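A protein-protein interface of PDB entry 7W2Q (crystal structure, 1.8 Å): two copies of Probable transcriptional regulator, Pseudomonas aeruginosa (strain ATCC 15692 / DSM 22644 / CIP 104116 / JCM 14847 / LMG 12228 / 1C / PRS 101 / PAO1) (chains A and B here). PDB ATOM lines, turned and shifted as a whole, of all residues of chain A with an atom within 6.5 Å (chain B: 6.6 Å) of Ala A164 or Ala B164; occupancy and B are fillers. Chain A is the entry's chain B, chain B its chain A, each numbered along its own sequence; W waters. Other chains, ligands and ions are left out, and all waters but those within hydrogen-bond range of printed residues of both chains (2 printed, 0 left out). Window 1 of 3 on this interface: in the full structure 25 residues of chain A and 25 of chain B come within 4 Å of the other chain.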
ATOM      1  N   TYR A 159      28.220 -12.812 -34.386  1.00  0.00           N
ATOM      2  CA  TYR A 159      27.453 -11.605 -34.681  1.00  0.00           C
ATOM      3  C   TYR A 159      26.275 -11.467 -33.730  1.00  0.00           C
ATOM      4  O   TYR A 159      25.996 -10.374 -33.213  1.00  0.00           O
ATOM      5  CB  TYR A 159      26.961 -11.635 -36.132  1.00  0.00           C
ATOM      6  CG  TYR A 159      26.192 -10.389 -36.515  1.00  0.00           C
ATOM      7  CD1 TYR A 159      24.823 -10.288 -36.280  1.00  0.00           C
ATOM      8  CD2 TYR A 159      26.841  -9.304 -37.085  1.00  0.00           C
ATOM      9  CE1 TYR A 159      24.114  -9.143 -36.617  1.00  0.00           C
ATOM     10  CE2 TYR A 159      26.142  -8.153 -37.427  1.00  0.00           C
ATOM     11  CZ  TYR A 159      24.786  -8.082 -37.191  1.00  0.00           C
ATOM     12  OH  TYR A 159      24.108  -6.946 -37.520  1.00  0.00           O
ATOM     13  N   CYS A 160      25.534 -12.561 -33.521  1.00  0.00           N
ATOM     14  CA  CYS A 160      24.329 -12.482 -32.698  1.00  0.00           C
ATOM     15  C   CYS A 160      24.678 -12.270 -31.234  1.00  0.00           C
ATOM     16  O   CYS A 160      23.954 -11.565 -30.520  1.00  0.00           O
ATOM     17  CB  CYS A 160      23.481 -13.740 -32.874  1.00  0.00           C
ATOM     18  SG  CYS A 160      22.642 -13.840 -34.466  1.00  0.00           S
ATOM     19  N   ALA A 161      25.783 -12.866 -30.768  1.00  0.00           N
ATOM     20  CA  ALA A 161      26.212 -12.608 -29.394  1.00  0.00           C
ATOM     21  C   ALA A 161      26.541 -11.133 -29.195  1.00  0.00           C
ATOM     22  O   ALA A 161      26.167 -10.535 -28.178  1.00  0.00           O
ATOM     23  CB  ALA A 161      27.411 -13.485 -29.044  1.00  0.00           C
ATOM     24  N   ALA A 162      27.245 -10.533 -30.157  1.00  0.00           N
ATOM     25  CA  ALA A 162      27.583  -9.117 -30.063  1.00  0.00           C
ATOM     26  C   ALA A 162      26.325  -8.263 -30.079  1.00  0.00           C
ATOM     27  O   ALA A 162      26.209  -7.300 -29.315  1.00  0.00           O
ATOM     28  CB  ALA A 162      28.509  -8.709 -31.207  1.00  0.00           C
ATOM     29  N   TRP A 163      25.382  -8.597 -30.958  1.00  0.00           N
ATOM     30  CA  TRP A 163      24.128  -7.852 -30.993  1.00  0.00           C
ATOM     31  C   TRP A 163      23.405  -7.937 -29.651  1.00  0.00           C
ATOM     32  O   TRP A 163      22.890  -6.932 -29.145  1.00  0.00           O
ATOM     33  CB  TRP A 163      23.239  -8.384 -32.116  1.00  0.00           C
ATOM     34  CG  TRP A 163      22.033  -7.518 -32.311  1.00  0.00           C
ATOM     35  CD1 TRP A 163      21.895  -6.487 -33.193  1.00  0.00           C
ATOM     36  CD2 TRP A 163      20.811  -7.575 -31.565  1.00  0.00           C
ATOM     37  NE1 TRP A 163      20.653  -5.910 -33.060  1.00  0.00           N
ATOM     38  CE2 TRP A 163      19.972  -6.558 -32.061  1.00  0.00           C
ATOM     39  CE3 TRP A 163      20.341  -8.390 -30.533  1.00  0.00           C
ATOM     40  CZ2 TRP A 163      18.692  -6.343 -31.565  1.00  0.00           C
ATOM     41  CZ3 TRP A 163      19.067  -8.161 -30.029  1.00  0.00           C
ATOM     42  CH2 TRP A 163      18.265  -7.153 -30.551  1.00  0.00           C
ATOM     43  N   ALA A 164      23.373  -9.126 -29.054  1.00  0.00           N
ATOM     44  CA  ALA A 164      22.675  -9.316 -27.788  1.00  0.00           C
ATOM     45  C   ALA A 164      23.333  -8.511 -26.672  1.00  0.00           C
ATOM     46  O   ALA A 164      22.655  -7.833 -25.891  1.00  0.00           O
ATOM     47  CB  ALA A 164      22.640 -10.806 -27.437  1.00  0.00           C
ATOM     48  N   LEU A 165      24.661  -8.573 -26.575  1.00  0.00           N
ATOM     49  CA  LEU A 165      25.341  -7.838 -25.506  1.00  0.00           C
ATOM     50  C   LEU A 165      25.089  -6.335 -25.622  1.00  0.00           C
ATOM     51  O   LEU A 165      24.757  -5.665 -24.622  1.00  0.00           O
ATOM     52  CB  LEU A 165      26.847  -8.161 -25.527  1.00  0.00           C
ATOM     53  CG  LEU A 165      27.657  -7.427 -24.455  1.00  0.00           C
ATOM     54  CD1 LEU A 165      27.274  -7.928 -23.073  1.00  0.00           C
ATOM     55  CD2 LEU A 165      29.165  -7.633 -24.719  1.00  0.00           C
ATOM     56  N   VAL A 166      25.175  -5.796 -26.841  1.00  0.00           N
ATOM     57  CA  VAL A 166      24.954  -4.366 -27.046  1.00  0.00           C
ATOM     58  C   VAL A 166      23.517  -3.992 -26.682  1.00  0.00           C
ATOM     59  O   VAL A 166      23.277  -3.003 -25.979  1.00  0.00           O
ATOM     60  CB  VAL A 166      25.287  -3.970 -28.498  1.00  0.00           C
ATOM     61  CG1 VAL A 166      24.817  -2.552 -28.778  1.00  0.00           C
ATOM     62  CG2 VAL A 166      26.783  -4.078 -28.756  1.00  0.00           C
ATOM     63  N   HIS A 167      22.546  -4.776 -27.160  1.00  0.00           N
ATOM     64  CA  HIS A 167      21.135  -4.474 -26.882  1.00  0.00           C
ATOM     65  C   HIS A 167      20.846  -4.478 -25.384  1.00  0.00           C
ATOM     66  O   HIS A 167      20.177  -3.571 -24.859  1.00  0.00           O
ATOM     67  CB  HIS A 167      20.242  -5.488 -27.584  1.00  0.00           C
ATOM     68  CG  HIS A 167      18.782  -5.182 -27.460  1.00  0.00           C
ATOM     69  ND1 HIS A 167      18.137  -4.286 -28.283  1.00  0.00           N
ATOM     70  CD2 HIS A 167      17.848  -5.649 -26.599  1.00  0.00           C
ATOM     71  CE1 HIS A 167      16.861  -4.219 -27.942  1.00  0.00           C
ATOM     72  NE2 HIS A 167      16.659  -5.036 -26.923  1.00  0.00           N
ATOM     73  N   GLY A 168      21.327  -5.503 -24.682  1.00  0.00           N
ATOM     74  CA  GLY A 168      21.107  -5.567 -23.245  1.00  0.00           C
ATOM     75  C   GLY A 168      21.850  -4.486 -22.491  1.00  0.00           C
ATOM     76  O   GLY A 168      21.359  -3.976 -21.482  1.00  0.00           O
ATOM     77  N   ALA A 169      23.048  -4.128 -22.960  1.00  0.00           N
ATOM     78  CA  ALA A 169      23.806  -3.069 -22.299  1.00  0.00           C
ATOM     79  C   ALA A 169      23.079  -1.735 -22.403  1.00  0.00           C
ATOM     80  O   ALA A 169      23.016  -0.967 -21.436  1.00  0.00           O
ATOM     81  CB  ALA A 169      25.206  -2.963 -22.901  1.00  0.00           C
ATOM     82  N   VAL A 170      22.508  -1.442 -23.570  1.00  0.00           N
ATOM     83  CA  VAL A 170      21.730  -0.215 -23.708  1.00  0.00           C
ATOM     84  C   VAL A 170      20.551  -0.221 -22.745  1.00  0.00           C
ATOM     85  O   VAL A 170      20.236   0.797 -22.119  1.00  0.00           O
ATOM     86  CB  VAL A 170      21.268  -0.039 -25.169  1.00  0.00           C
ATOM     87  CG1 VAL A 170      20.230   1.065 -25.266  1.00  0.00           C
ATOM     88  CG2 VAL A 170      22.472   0.253 -26.069  1.00  0.00           C
ATOM     89  N   LEU A 172      20.343  -1.656 -19.883  1.00  0.00           N
ATOM     90  CA  LEU A 172      20.855  -1.407 -18.536  1.00  0.00           C
ATOM     91  C   LEU A 172      20.819   0.071 -18.201  1.00  0.00           C
ATOM     92  O   LEU A 172      20.410   0.463 -17.098  1.00  0.00           O
ATOM     93  CB  LEU A 172      22.287  -1.936 -18.452  1.00  0.00           C
ATOM     94  CG  LEU A 172      22.961  -2.590 -17.263  1.00  0.00           C
ATOM     95  CD1 LEU A 172      22.047  -3.557 -16.500  1.00  0.00           C
ATOM     96  CD2 LEU A 172      24.199  -3.302 -17.786  1.00  0.00           C
ATOM     97  N   LEU A 192      32.389  -3.783 -19.499  1.00  0.00           N
ATOM     98  CA  LEU A 192      31.505  -4.255 -20.564  1.00  0.00           C
ATOM     99  C   LEU A 192      32.241  -4.351 -21.899  1.00  0.00           C
ATOM    100  O   LEU A 192      32.025  -5.297 -22.671  1.00  0.00           O
ATOM    101  CB  LEU A 192      30.305  -3.311 -20.670  1.00  0.00           C
ATOM    102  CG  LEU A 192      28.893  -3.884 -20.718  1.00  0.00           C
ATOM    103  CD1 LEU A 192      28.722  -5.020 -19.718  1.00  0.00           C
ATOM    104  CD2 LEU A 192      27.894  -2.772 -20.418  1.00  0.00           C
ATOM    105  N   TYR B 159      26.775  -8.890 -12.001  1.00  0.00           N
ATOM    106  CA  TYR B 159      25.321  -8.985 -12.043  1.00  0.00           C
ATOM    107  C   TYR B 159      24.760  -8.244 -13.252  1.00  0.00           C
ATOM    108  O   TYR B 159      23.893  -8.761 -13.977  1.00  0.00           O
ATOM    109  CB  TYR B 159      24.737  -8.426 -10.748  1.00  0.00           C
ATOM    110  CG  TYR B 159      23.232  -8.521 -10.689  1.00  0.00           C
ATOM    111  CD1 TYR B 159      22.426  -7.533 -11.254  1.00  0.00           C
ATOM    112  CD2 TYR B 159      22.610  -9.606 -10.082  1.00  0.00           C
ATOM    113  CE1 TYR B 159      21.047  -7.620 -11.207  1.00  0.00           C
ATOM    114  CE2 TYR B 159      21.229  -9.704 -10.038  1.00  0.00           C
ATOM    115  CZ  TYR B 159      20.458  -8.709 -10.598  1.00  0.00           C
ATOM    116  OH  TYR B 159      19.089  -8.802 -10.546  1.00  0.00           O
ATOM    117  N   CYS B 160      25.245  -7.024 -13.490  1.00  0.00           N
ATOM    118  CA  CYS B 160      24.704  -6.222 -14.586  1.00  0.00           C
ATOM    119  C   CYS B 160      25.090  -6.791 -15.948  1.00  0.00           C
ATOM    120  O   CYS B 160      24.294  -6.729 -16.902  1.00  0.00           O
ATOM    121  CB  CYS B 160      25.168  -4.772 -14.436  1.00  0.00           C
ATOM    122  SG  CYS B 160      24.341  -3.906 -13.093  1.00  0.00           S
ATOM    123  N   ALA B 161      26.299  -7.345 -16.071  1.00  0.00           N
ATOM    124  CA  ALA B 161      26.673  -8.008 -17.319  1.00  0.00           C
ATOM    125  C   ALA B 161      25.751  -9.188 -17.601  1.00  0.00           C
ATOM    126  O   ALA B 161      25.285  -9.375 -18.736  1.00  0.00           O
ATOM    127  CB  ALA B 161      28.137  -8.468 -17.257  1.00  0.00           C
ATOM    128  N   ALA B 162      25.458  -9.989 -16.573  1.00  0.00           N
ATOM    129  CA  ALA B 162      24.559 -11.126 -16.747  1.00  0.00           C
ATOM    130  C   ALA B 162      23.168 -10.666 -17.161  1.00  0.00           C
ATOM    131  O   ALA B 162      22.551 -11.250 -18.061  1.00  0.00           O
ATOM    132  CB  ALA B 162      24.491 -11.946 -15.451  1.00  0.00           C
ATOM    133  N   TRP B 163      22.666  -9.616 -16.525  1.00  0.00           N
ATOM    134  CA  TRP B 163      21.361  -9.082 -16.896  1.00  0.00           C
ATOM    135  C   TRP B 163      21.353  -8.633 -18.350  1.00  0.00           C
ATOM    136  O   TRP B 163      20.385  -8.884 -19.081  1.00  0.00           O
ATOM    137  CB  TRP B 163      20.996  -7.925 -15.959  1.00  0.00           C
ATOM    138  CG  TRP B 163      19.569  -7.480 -16.163  1.00  0.00           C
ATOM    139  CD1 TRP B 163      18.474  -7.893 -15.461  1.00  0.00           C
ATOM    140  CD2 TRP B 163      19.084  -6.580 -17.172  1.00  0.00           C
ATOM    141  NE1 TRP B 163      17.340  -7.292 -15.955  1.00  0.00           N
ATOM    142  CE2 TRP B 163      17.687  -6.484 -17.007  1.00  0.00           C
ATOM    143  CE3 TRP B 163      19.694  -5.841 -18.189  1.00  0.00           C
ATOM    144  CZ2 TRP B 163      16.895  -5.672 -17.817  1.00  0.00           C
ATOM    145  CZ3 TRP B 163      18.915  -5.041 -18.985  1.00  0.00           C
ATOM    146  CH2 TRP B 163      17.524  -4.963 -18.801  1.00  0.00           C
ATOM    147  N   ALA B 164      22.424  -7.967 -18.789  1.00  0.00           N
ATOM    148  CA  ALA B 164      22.470  -7.451 -20.152  1.00  0.00           C
ATOM    149  C   ALA B 164      22.454  -8.584 -21.165  1.00  0.00           C
ATOM    150  O   ALA B 164      21.719  -8.535 -22.156  1.00  0.00           O
ATOM    151  CB  ALA B 164      23.713  -6.577 -20.339  1.00  0.00           C
ATOM    152  N   LEU B 165      23.272  -9.615 -20.942  1.00  0.00           N
ATOM    153  CA  LEU B 165      23.334 -10.726 -21.890  1.00  0.00           C
ATOM    154  C   LEU B 165      21.978 -11.406 -22.032  1.00  0.00           C
ATOM    155  O   LEU B 165      21.516 -11.671 -23.150  1.00  0.00           O
ATOM    156  CB  LEU B 165      24.398 -11.726 -21.433  1.00  0.00           C
ATOM    157  CG  LEU B 165      24.556 -12.915 -22.382  1.00  0.00           C
ATOM    158  CD1 LEU B 165      25.147 -12.456 -23.704  1.00  0.00           C
ATOM    159  CD2 LEU B 165      25.425 -13.965 -21.718  1.00  0.00           C
ATOM    160  N   VAL B 166      21.304 -11.653 -20.903  1.00  0.00           N
ATOM    161  CA  VAL B 166      19.997 -12.301 -20.940  1.00  0.00           C
ATOM    162  C   VAL B 166      18.988 -11.418 -21.665  1.00  0.00           C
ATOM    163  O   VAL B 166      18.243 -11.881 -22.539  1.00  0.00           O
ATOM    164  CB  VAL B 166      19.532 -12.641 -19.514  1.00  0.00           C
ATOM    165  CG1 VAL B 166      18.088 -13.118 -19.515  1.00  0.00           C
ATOM    166  CG2 VAL B 166      20.441 -13.699 -18.899  1.00  0.00           C
ATOM    167  N   HIS B 167      18.942 -10.131 -21.308  1.00  0.00           N
ATOM    168  CA  HIS B 167      17.989  -9.221 -21.953  1.00  0.00           C
ATOM    169  C   HIS B 167      18.205  -9.163 -23.464  1.00  0.00           C
ATOM    170  O   HIS B 167      17.236  -9.202 -24.242  1.00  0.00           O
ATOM    171  CB  HIS B 167      18.109  -7.826 -21.347  1.00  0.00           C
ATOM    172  CG  HIS B 167      17.027  -6.895 -21.784  1.00  0.00           C
ATOM    173  ND1 HIS B 167      15.769  -6.914 -21.229  1.00  0.00           N
ATOM    174  CD2 HIS B 167      17.005  -5.941 -22.742  1.00  0.00           C
ATOM    175  CE1 HIS B 167      15.018  -5.993 -21.813  1.00  0.00           C
ATOM    176  NE2 HIS B 167      15.743  -5.395 -22.744  1.00  0.00           N
ATOM    177  N   GLY B 168      19.467  -9.065 -23.897  1.00  0.00           N
ATOM    178  CA  GLY B 168      19.754  -9.023 -25.323  1.00  0.00           C
ATOM    179  C   GLY B 168      19.471 -10.334 -26.025  1.00  0.00           C
ATOM    180  O   GLY B 168      19.033 -10.350 -27.182  1.00  0.00           O
ATOM    181  N   ALA B 169      19.733 -11.451 -25.349  1.00  0.00           N
ATOM    182  CA  ALA B 169      19.455 -12.752 -25.953  1.00  0.00           C
ATOM    183  C   ALA B 169      17.958 -12.940 -26.171  1.00  0.00           C
ATOM    184  O   ALA B 169      17.529 -13.436 -27.220  1.00  0.00           O
ATOM    185  CB  ALA B 169      20.031 -13.869 -25.078  1.00  0.00           C
ATOM    186  N   VAL B 170      17.139 -12.535 -25.195  1.00  0.00           N
ATOM    187  CA  VAL B 170      15.692 -12.632 -25.374  1.00  0.00           C
ATOM    188  C   VAL B 170      15.243 -11.794 -26.563  1.00  0.00           C
ATOM    189  O   VAL B 170      14.406 -12.222 -27.370  1.00  0.00           O
ATOM    190  CB  VAL B 170      14.976 -12.219 -24.080  1.00  0.00           C
ATOM    191  CG1 VAL B 170      13.496 -11.922 -24.352  1.00  0.00           C
ATOM    192  CG2 VAL B 170      15.153 -13.308 -23.015  1.00  0.00           C
ATOM    193  N   LEU B 172      16.969 -11.064 -29.150  1.00  0.00           N
ATOM    194  CA  LEU B 172      17.411 -11.770 -30.345  1.00  0.00           C
ATOM    195  C   LEU B 172      16.335 -12.714 -30.853  1.00  0.00           C
ATOM    196  O   LEU B 172      16.045 -12.755 -32.058  1.00  0.00           O
ATOM    197  CB  LEU B 172      18.699 -12.529 -30.001  1.00  0.00           C
ATOM    198  CG  LEU B 172      19.676 -13.020 -31.050  1.00  0.00           C
ATOM    199  CD1 LEU B 172      20.020 -11.928 -32.055  1.00  0.00           C
ATOM    200  CD2 LEU B 172      20.919 -13.506 -30.303  1.00  0.00           C
ATOM    201  N   LEU B 192      25.565 -19.400 -26.446  1.00  0.00           N
ATOM    202  CA  LEU B 192      25.226 -18.278 -25.568  1.00  0.00           C
ATOM    203  C   LEU B 192      25.428 -18.647 -24.103  1.00  0.00           C
ATOM    204  O   LEU B 192      25.903 -17.822 -23.307  1.00  0.00           O
ATOM    205  CB  LEU B 192      23.783 -17.828 -25.813  1.00  0.00           C
ATOM    206  CG  LEU B 192      23.542 -16.879 -26.988  1.00  0.00           C
ATOM    207  CD1 LEU B 192      22.082 -16.456 -27.015  1.00  0.00           C
ATOM    208  CD2 LEU B 192      24.455 -15.656 -26.929  1.00  0.00           C
HETATM  209  O   HOH W   1      15.363  -2.971 -24.546  1.00  0.00           O
HETATM  210  O   HOH W   2      14.148  -5.857 -25.746  1.00  0.00           O
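Water W2 bridges a ring nitrogen (NE2) of His A167 and a ring nitrogen (NE2) of His B167. Water W1 bridges NE2 of His B167 (3.0 Å) and NE2 of His A167 (3.4 Å).
Leu B172 touches Cys A160 (CD2 to O, 3.6 Å). Trp A163 touches Gly B168 (CZ3 to O, 3.6 Å). Trp A163 touches Leu B172. Ala A164 touches Gly B168 (O to CA, 3.2 Å). Ala A164 touches Ala B169 (CB to N, 3.6 Å). His B167 touches His A167 (CD2 to CD2, 3.96 Å). Gly A168 touches Trp B163. O of Ala B164 touches CA of Gly A168, 3.2 Å away. Gly A168 touches Gly B168 (N to CA, 3.9 Å). Cys B160 touches Leu A172 (O to CD2, 3.5 Å).
Trp A163 touches Gly B168, and with the chains exchanged Gly A168 touches Trp B163. Trp A163 touches Leu B172, and with the chains exchanged Leu A172 touches Trp B163. Ala A164 touches Gly B168, and with the chains exchanged Gly A168 touches Ala B164. Gly B168 touches its own counterpart, Gly A168. Positions printed for both chains: 159, 160, 161, 162, 163, 164, 165, 166, 167, 168, 169, 170, 172 and 192. Of the 13 pairs that touch across the chains among the printed residues, 13 have their exchanged pair printed and touching as well.
Along chain A the printed residues that touch a printed residue of chain B span positions 160 to 172. Of the 14 printed residues of chain B, 7 touch a printed residue of chain A.
Of chain A, only Ala A164, Gly A168 and Ala A169 come within 4 Å of Ala B164. Of the printed residues of chain B, Gly A168 touches Trp B163 (3.7 Å), Ala B164 (3.2 Å) and Gly B168 (3.9 Å). Of the printed residues of chain A, His B167 touches His A167. Of the printed residues of chain A, Gly B168 touches Trp A163, Ala A164 and Gly A168. Ala B162 touches none of the printed residues of chain A. The nearest printed residue of chain A that does not touch His B167 is Gly A168 (4.1 Å).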
